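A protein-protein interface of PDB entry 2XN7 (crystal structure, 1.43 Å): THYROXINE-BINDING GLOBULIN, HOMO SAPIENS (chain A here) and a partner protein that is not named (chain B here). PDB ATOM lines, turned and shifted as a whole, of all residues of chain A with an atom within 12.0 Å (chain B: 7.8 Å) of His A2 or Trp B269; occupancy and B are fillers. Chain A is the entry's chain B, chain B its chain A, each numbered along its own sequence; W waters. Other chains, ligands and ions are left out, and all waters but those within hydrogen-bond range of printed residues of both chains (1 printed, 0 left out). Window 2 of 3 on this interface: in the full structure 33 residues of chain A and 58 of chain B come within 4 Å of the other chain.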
ATOM      1  N   HIS A   2     -15.498   2.442 -11.767  1.00  0.00           N
ATOM      2  CA  HIS A   2     -14.407   1.612 -11.193  1.00  0.00           C
ATOM      3  C   HIS A   2     -14.891   0.932  -9.910  1.00  0.00           C
ATOM      4  O   HIS A   2     -15.679   1.515  -9.168  1.00  0.00           O
ATOM      5  CB  HIS A   2     -13.184   2.476 -10.891  1.00  0.00           C
ATOM      6  CG  HIS A   2     -12.722   3.301 -12.052  1.00  0.00           C
ATOM      7  ND1 HIS A   2     -12.592   2.786 -13.324  1.00  0.00           N
ATOM      8  CD2 HIS A   2     -12.342   4.598 -12.133  1.00  0.00           C
ATOM      9  CE1 HIS A   2     -12.162   3.732 -14.140  1.00  0.00           C
ATOM     10  NE2 HIS A   2     -11.999   4.840 -13.441  1.00  0.00           N
ATOM     11  N   PRO A   3     -14.418  -0.298  -9.640  1.00  0.00           N
ATOM     12  CA  PRO A   3     -14.799  -0.981  -8.411  1.00  0.00           C
ATOM     13  C   PRO A   3     -14.321  -0.246  -7.166  1.00  0.00           C
ATOM     14  O   PRO A   3     -13.230   0.332  -7.157  1.00  0.00           O
ATOM     15  CB  PRO A   3     -14.079  -2.325  -8.524  1.00  0.00           C
ATOM     16  CG  PRO A   3     -12.927  -2.043  -9.411  1.00  0.00           C
ATOM     17  CD  PRO A   3     -13.457  -1.094 -10.419  1.00  0.00           C
ATOM     18  N   ILE A   4     -15.155  -0.273  -6.135  1.00  0.00           N
ATOM     19  CA  ILE A   4     -14.833   0.291  -4.835  1.00  0.00           C
ATOM     20  C   ILE A   4     -14.354  -0.820  -3.926  1.00  0.00           C
ATOM     21  O   ILE A   4     -15.006  -1.880  -3.828  1.00  0.00           O
ATOM     22  CB  ILE A   4     -16.068   0.962  -4.197  1.00  0.00           C
ATOM     23  CG1 ILE A   4     -16.561   2.108  -5.085  1.00  0.00           C
ATOM     24  CG2 ILE A   4     -15.746   1.440  -2.778  1.00  0.00           C
ATOM     25  CD1 ILE A   4     -17.950   2.592  -4.751  1.00  0.00           C
ATOM     26  N   ILE A   5     -13.220  -0.583  -3.268  1.00  0.00           N
ATOM     27  CA  ILE A   5     -12.741  -1.467  -2.216  1.00  0.00           C
ATOM     28  C   ILE A   5     -12.620  -0.624  -0.960  1.00  0.00           C
ATOM     29  O   ILE A   5     -11.821   0.307  -0.914  1.00  0.00           O
ATOM     30  CB  ILE A   5     -11.395  -2.139  -2.577  1.00  0.00           C
ATOM     31  CG1 ILE A   5     -11.580  -3.091  -3.771  1.00  0.00           C
ATOM     32  CG2 ILE A   5     -10.846  -2.917  -1.377  1.00  0.00           C
ATOM     33  CD1 ILE A   5     -10.297  -3.705  -4.298  1.00  0.00           C
ATOM     34  N   GLN A   6     -13.469  -0.922   0.025  1.00  0.00           N
ATOM     35  CA  GLN A   6     -13.518  -0.162   1.265  1.00  0.00           C
ATOM     36  C   GLN A   6     -13.090  -1.074   2.396  1.00  0.00           C
ATOM     37  O   GLN A   6     -13.817  -1.997   2.769  1.00  0.00           O
ATOM     38  CB  GLN A   6     -14.919   0.336   1.563  1.00  0.00           C
ATOM     39  CG  GLN A   6     -15.426   1.359   0.632  1.00  0.00           C
ATOM     40  CD  GLN A   6     -16.738   1.920   1.110  1.00  0.00           C
ATOM     41  OE1 GLN A   6     -17.799   1.436   0.726  1.00  0.00           O
ATOM     42  NE2 GLN A   6     -16.671   2.898   2.004  1.00  0.00           N
ATOM     43  N   GLN B 209      -7.930   7.012  -2.130  1.00  0.00           N
ATOM     44  CA  GLN B 209      -7.404   7.368  -3.425  1.00  0.00           C
ATOM     45  C   GLN B 209      -7.989   6.478  -4.498  1.00  0.00           C
ATOM     46  O   GLN B 209      -8.566   5.442  -4.220  1.00  0.00           O
ATOM     47  CB  GLN B 209      -5.870   7.362  -3.449  1.00  0.00           C
ATOM     48  CG  GLN B 209      -5.144   6.060  -3.403  1.00  0.00           C
ATOM     49  CD  GLN B 209      -3.623   6.329  -3.574  1.00  0.00           C
ATOM     50  OE1 GLN B 209      -3.186   6.839  -4.609  1.00  0.00           O
ATOM     51  NE2 GLN B 209      -2.860   6.027  -2.577  1.00  0.00           N
ATOM     52  N   MET B 210      -7.847   6.930  -5.733  1.00  0.00           N
ATOM     53  CA  MET B 210      -8.354   6.234  -6.902  1.00  0.00           C
ATOM     54  C   MET B 210      -7.149   6.002  -7.791  1.00  0.00           C
ATOM     55  O   MET B 210      -6.675   6.930  -8.421  1.00  0.00           O
ATOM     56  CB  MET B 210      -9.417   7.086  -7.611  1.00  0.00           C
ATOM     57  CG  MET B 210     -10.667   7.398  -6.772  1.00  0.00           C
ATOM     58  SD  MET B 210     -11.626   8.847  -7.319  1.00  0.00           S
ATOM     59  CE  MET B 210     -13.113   8.698  -6.322  1.00  0.00           C
ATOM     60  N   GLU B 211      -6.638   4.771  -7.821  1.00  0.00           N
ATOM     61  CA  GLU B 211      -5.415   4.450  -8.541  1.00  0.00           C
ATOM     62  C   GLU B 211      -5.545   3.055  -9.132  1.00  0.00           C
ATOM     63  O   GLU B 211      -6.479   2.325  -8.784  1.00  0.00           O
ATOM     64  CB  GLU B 211      -4.228   4.494  -7.581  1.00  0.00           C
ATOM     65  CG  GLU B 211      -2.889   4.498  -8.264  1.00  0.00           C
ATOM     66  CD  GLU B 211      -2.897   5.293  -9.557  1.00  0.00           C
ATOM     67  OE1 GLU B 211      -2.595   4.690 -10.625  1.00  0.00           O
ATOM     68  OE2 GLU B 211      -3.199   6.521  -9.513  1.00  0.00           O
ATOM     69  N   GLN B 212      -4.612   2.688 -10.008  1.00  0.00           N
ATOM     70  CA  GLN B 212      -4.545   1.335 -10.536  1.00  0.00           C
ATOM     71  C   GLN B 212      -3.761   0.464  -9.568  1.00  0.00           C
ATOM     72  O   GLN B 212      -2.605   0.774  -9.234  1.00  0.00           O
ATOM     73  CB  GLN B 212      -3.855   1.306 -11.887  1.00  0.00           C
ATOM     74  CG  GLN B 212      -4.608   2.000 -12.990  1.00  0.00           C
ATOM     75  CD  GLN B 212      -3.897   1.894 -14.329  1.00  0.00           C
ATOM     76  OE1 GLN B 212      -2.763   1.410 -14.407  1.00  0.00           O
ATOM     77  NE2 GLN B 212      -4.542   2.360 -15.382  1.00  0.00           N
ATOM     78  N   TYR B 213      -4.383  -0.636  -9.141  1.00  0.00           N
ATOM     79  CA  TYR B 213      -3.778  -1.605  -8.258  1.00  0.00           C
ATOM     80  C   TYR B 213      -4.046  -3.011  -8.797  1.00  0.00           C
ATOM     81  O   TYR B 213      -5.112  -3.275  -9.380  1.00  0.00           O
ATOM     82  CB  TYR B 213      -4.396  -1.533  -6.849  1.00  0.00           C
ATOM     83  CG  TYR B 213      -4.210  -0.219  -6.075  1.00  0.00           C
ATOM     84  CD1 TYR B 213      -3.068   0.007  -5.369  1.00  0.00           C
ATOM     85  CD2 TYR B 213      -5.231   0.733  -6.010  1.00  0.00           C
ATOM     86  CE1 TYR B 213      -2.883   1.203  -4.653  1.00  0.00           C
ATOM     87  CE2 TYR B 213      -5.062   1.929  -5.286  1.00  0.00           C
ATOM     88  CZ  TYR B 213      -3.887   2.129  -4.599  1.00  0.00           C
ATOM     89  OH  TYR B 213      -3.683   3.303  -3.885  1.00  0.00           O
ATOM     90  N   TYR B 214      -3.116  -3.909  -8.536  1.00  0.00           N
ATOM     91  CA  TYR B 214      -3.377  -5.338  -8.728  1.00  0.00           C
ATOM     92  C   TYR B 214      -4.411  -5.766  -7.693  1.00  0.00           C
ATOM     93  O   TYR B 214      -4.244  -5.544  -6.489  1.00  0.00           O
ATOM     94  CB  TYR B 214      -2.089  -6.138  -8.560  1.00  0.00           C
ATOM     95  CG  TYR B 214      -1.166  -6.101  -9.737  1.00  0.00           C
ATOM     96  CD1 TYR B 214      -1.362  -6.935 -10.821  1.00  0.00           C
ATOM     97  CD2 TYR B 214      -0.095  -5.233  -9.773  1.00  0.00           C
ATOM     98  CE1 TYR B 214      -0.518  -6.923 -11.919  1.00  0.00           C
ATOM     99  CE2 TYR B 214       0.753  -5.187 -10.876  1.00  0.00           C
ATOM    100  CZ  TYR B 214       0.545  -6.041 -11.942  1.00  0.00           C
ATOM    101  OH  TYR B 214       1.430  -5.972 -13.016  1.00  0.00           O
ATOM    102  N   HIS B 215      -5.479  -6.441  -8.155  1.00  0.00           N
ATOM    103  CA  HIS B 215      -6.534  -6.910  -7.252  1.00  0.00           C
ATOM    104  C   HIS B 215      -7.275  -8.061  -7.895  1.00  0.00           C
ATOM    105  O   HIS B 215      -7.121  -8.323  -9.083  1.00  0.00           O
ATOM    106  CB  HIS B 215      -7.502  -5.773  -6.870  1.00  0.00           C
ATOM    107  CG  HIS B 215      -8.317  -5.263  -8.008  1.00  0.00           C
ATOM    108  ND1 HIS B 215      -9.657  -5.558  -8.167  1.00  0.00           N
ATOM    109  CD2 HIS B 215      -7.980  -4.470  -9.052  1.00  0.00           C
ATOM    110  CE1 HIS B 215     -10.104  -4.971  -9.263  1.00  0.00           C
ATOM    111  NE2 HIS B 215      -9.110  -4.301  -9.818  1.00  0.00           N
ATOM    112  N   GLN B 266      -4.787  -8.841 -11.184  1.00  0.00           N
ATOM    113  CA  GLN B 266      -4.774  -8.018 -12.383  1.00  0.00           C
ATOM    114  C   GLN B 266      -4.847  -6.552 -11.985  1.00  0.00           C
ATOM    115  O   GLN B 266      -5.618  -6.183 -11.106  1.00  0.00           O
ATOM    116  CB  GLN B 266      -5.924  -8.372 -13.353  1.00  0.00           C
ATOM    117  CG  GLN B 266      -5.703  -7.752 -14.749  1.00  0.00           C
ATOM    118  CD  GLN B 266      -6.846  -7.861 -15.746  1.00  0.00           C
ATOM    119  OE1 GLN B 266      -6.765  -7.314 -16.852  1.00  0.00           O
ATOM    120  NE2 GLN B 266      -7.923  -8.578 -15.383  1.00  0.00           N
ATOM    121  N   LYS B 267      -4.057  -5.725 -12.670  1.00  0.00           N
ATOM    122  CA  LYS B 267      -4.007  -4.312 -12.365  1.00  0.00           C
ATOM    123  C   LYS B 267      -5.125  -3.559 -13.067  1.00  0.00           C
ATOM    124  O   LYS B 267      -5.290  -3.658 -14.285  1.00  0.00           O
ATOM    125  CB  LYS B 267      -2.643  -3.743 -12.756  1.00  0.00           C
ATOM    126  CG  LYS B 267      -2.462  -2.307 -12.332  1.00  0.00           C
ATOM    127  CD  LYS B 267      -1.009  -1.836 -12.462  1.00  0.00           C
ATOM    128  CE  LYS B 267      -0.290  -1.767 -11.126  1.00  0.00           C
ATOM    129  NZ  LYS B 267       0.956  -0.946 -11.207  1.00  0.00           N
ATOM    130  N   GLY B 268      -5.882  -2.784 -12.304  1.00  0.00           N
ATOM    131  CA  GLY B 268      -6.923  -1.920 -12.844  1.00  0.00           C
ATOM    132  C   GLY B 268      -7.318  -0.854 -11.838  1.00  0.00           C
ATOM    133  O   GLY B 268      -6.898  -0.904 -10.676  1.00  0.00           O
ATOM    134  N   TRP B 269      -8.155   0.080 -12.262  1.00  0.00           N
ATOM    135  CA  TRP B 269      -8.605   1.162 -11.393  1.00  0.00           C
ATOM    136  C   TRP B 269      -9.404   0.653 -10.211  1.00  0.00           C
ATOM    137  O   TRP B 269     -10.286  -0.194 -10.380  1.00  0.00           O
ATOM    138  CB  TRP B 269      -9.443   2.172 -12.166  1.00  0.00           C
ATOM    139  CG  TRP B 269      -8.653   2.876 -13.208  1.00  0.00           C
ATOM    140  CD1 TRP B 269      -8.656   2.628 -14.539  1.00  0.00           C
ATOM    141  CD2 TRP B 269      -7.698   3.931 -12.998  1.00  0.00           C
ATOM    142  NE1 TRP B 269      -7.772   3.462 -15.180  1.00  0.00           N
ATOM    143  CE2 TRP B 269      -7.170   4.264 -14.255  1.00  0.00           C
ATOM    144  CE3 TRP B 269      -7.242   4.617 -11.873  1.00  0.00           C
ATOM    145  CZ2 TRP B 269      -6.221   5.257 -14.422  1.00  0.00           C
ATOM    146  CZ3 TRP B 269      -6.280   5.613 -12.046  1.00  0.00           C
ATOM    147  CH2 TRP B 269      -5.786   5.912 -13.311  1.00  0.00           C
ATOM    148  N   VAL B 270      -9.092   1.169  -9.029  1.00  0.00           N
ATOM    149  CA  VAL B 270      -9.860   0.893  -7.817  1.00  0.00           C
ATOM    150  C   VAL B 270     -10.093   2.218  -7.089  1.00  0.00           C
ATOM    151  O   VAL B 270      -9.175   3.040  -6.973  1.00  0.00           O
ATOM    152  CB  VAL B 270      -9.107  -0.057  -6.877  1.00  0.00           C
ATOM    153  CG1 VAL B 270      -9.902  -0.270  -5.577  1.00  0.00           C
ATOM    154  CG2 VAL B 270      -8.814  -1.385  -7.564  1.00  0.00           C
ATOM    155  N   ASP B 271     -11.318   2.434  -6.631  1.00  0.00           N
ATOM    156  CA  ASP B 271     -11.652   3.507  -5.704  1.00  0.00           C
ATOM    157  C   ASP B 271     -11.450   2.928  -4.300  1.00  0.00           C
ATOM    158  O   ASP B 271     -12.251   2.121  -3.821  1.00  0.00           O
ATOM    159  CB  ASP B 271     -13.104   3.914  -5.930  1.00  0.00           C
ATOM    160  CG  ASP B 271     -13.468   5.188  -5.239  1.00  0.00           C
ATOM    161  OD1 ASP B 271     -12.568   5.867  -4.712  1.00  0.00           O
ATOM    162  OD2 ASP B 271     -14.672   5.549  -5.270  1.00  0.00           O
ATOM    163  N   LEU B 272     -10.340   3.316  -3.679  1.00  0.00           N
ATOM    164  CA  LEU B 272      -9.793   2.623  -2.521  1.00  0.00           C
ATOM    165  C   LEU B 272      -9.877   3.429  -1.248  1.00  0.00           C
ATOM    166  O   LEU B 272      -9.456   4.570  -1.217  1.00  0.00           O
ATOM    167  CB  LEU B 272      -8.333   2.263  -2.791  1.00  0.00           C
ATOM    168  CG  LEU B 272      -7.557   1.565  -1.675  1.00  0.00           C
ATOM    169  CD1 LEU B 272      -8.194   0.219  -1.341  1.00  0.00           C
ATOM    170  CD2 LEU B 272      -6.086   1.392  -2.036  1.00  0.00           C
HETATM  171  O   HOH W   1     -16.025   4.728  -7.830  1.00  0.00           O
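The backbone carbonyl oxygen (O) of Pro A3 is in hydrogen-bond range of the backbone NH (N) of Asp B271 (2.9 Å). The backbone carbonyl oxygen (O) of Asp B271 is in hydrogen-bond range of the backbone NH (N) of Ile A5, at 2.9 Å.
Of the 5 printed residues of chain A, 4 touch a printed residue of chain B. Along chain A the printed residues that touch a printed residue of chain B span positions 2 to 5. Hydrophobic or aromatic side chains of chain B within 4 Å of the printed part of chain A: Trp B269, Val B270 and Leu B272. Among the printed residues, 8 pairs touch across the chains.
Water W1 lies within hydrogen-bond range of the side-chain carboxylate of Asp B271 (3.0 Å) and the backbone carbonyl oxygen of His A2 (3.5 Å).
His A2 touches just one residue of chain B: Trp B269 (3.4 Å). Pro A3 touches three residues of chain B. Of the printed residues of chain B, Ile A4 touches Asp B271. No residue of chain A comes within 4 Å of Met B210. No residue of chain A comes within 4 Å of Gly B268. Trp B269 touches just these residues of chain A: His A2 (3.4 Å) and Pro A3 (3.3 Å). Val B270 touches just these residues of chain A: Pro A3 and Ile A5. Of the printed residues of chain A, Leu B272 touches Ile A5 (3.5 Å). The nearest residue of chain B that does not touch His A2 is Asp B271 (4.7 Å).
Among the printed residues, pairs that only touch across the chains: His A2 with Trp B269, Pro A3 with Trp B269, Pro A3 with Val B270, Ile A4 with Asp B271, Ile A5 with Val B270 and Ile A5 with Leu B272.
N of Leu B272 lies within hydrogen-bond range of O of Gln B209 (2.8 Å). O of Glu B211 is in hydrogen-bond range of N of Val B270 (2.9 Å). The indole nitrogen (NE1) of Trp B269 lies close to the side-chain amide nitrogen (NE2) of Gln B212, 3.4 Å away.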
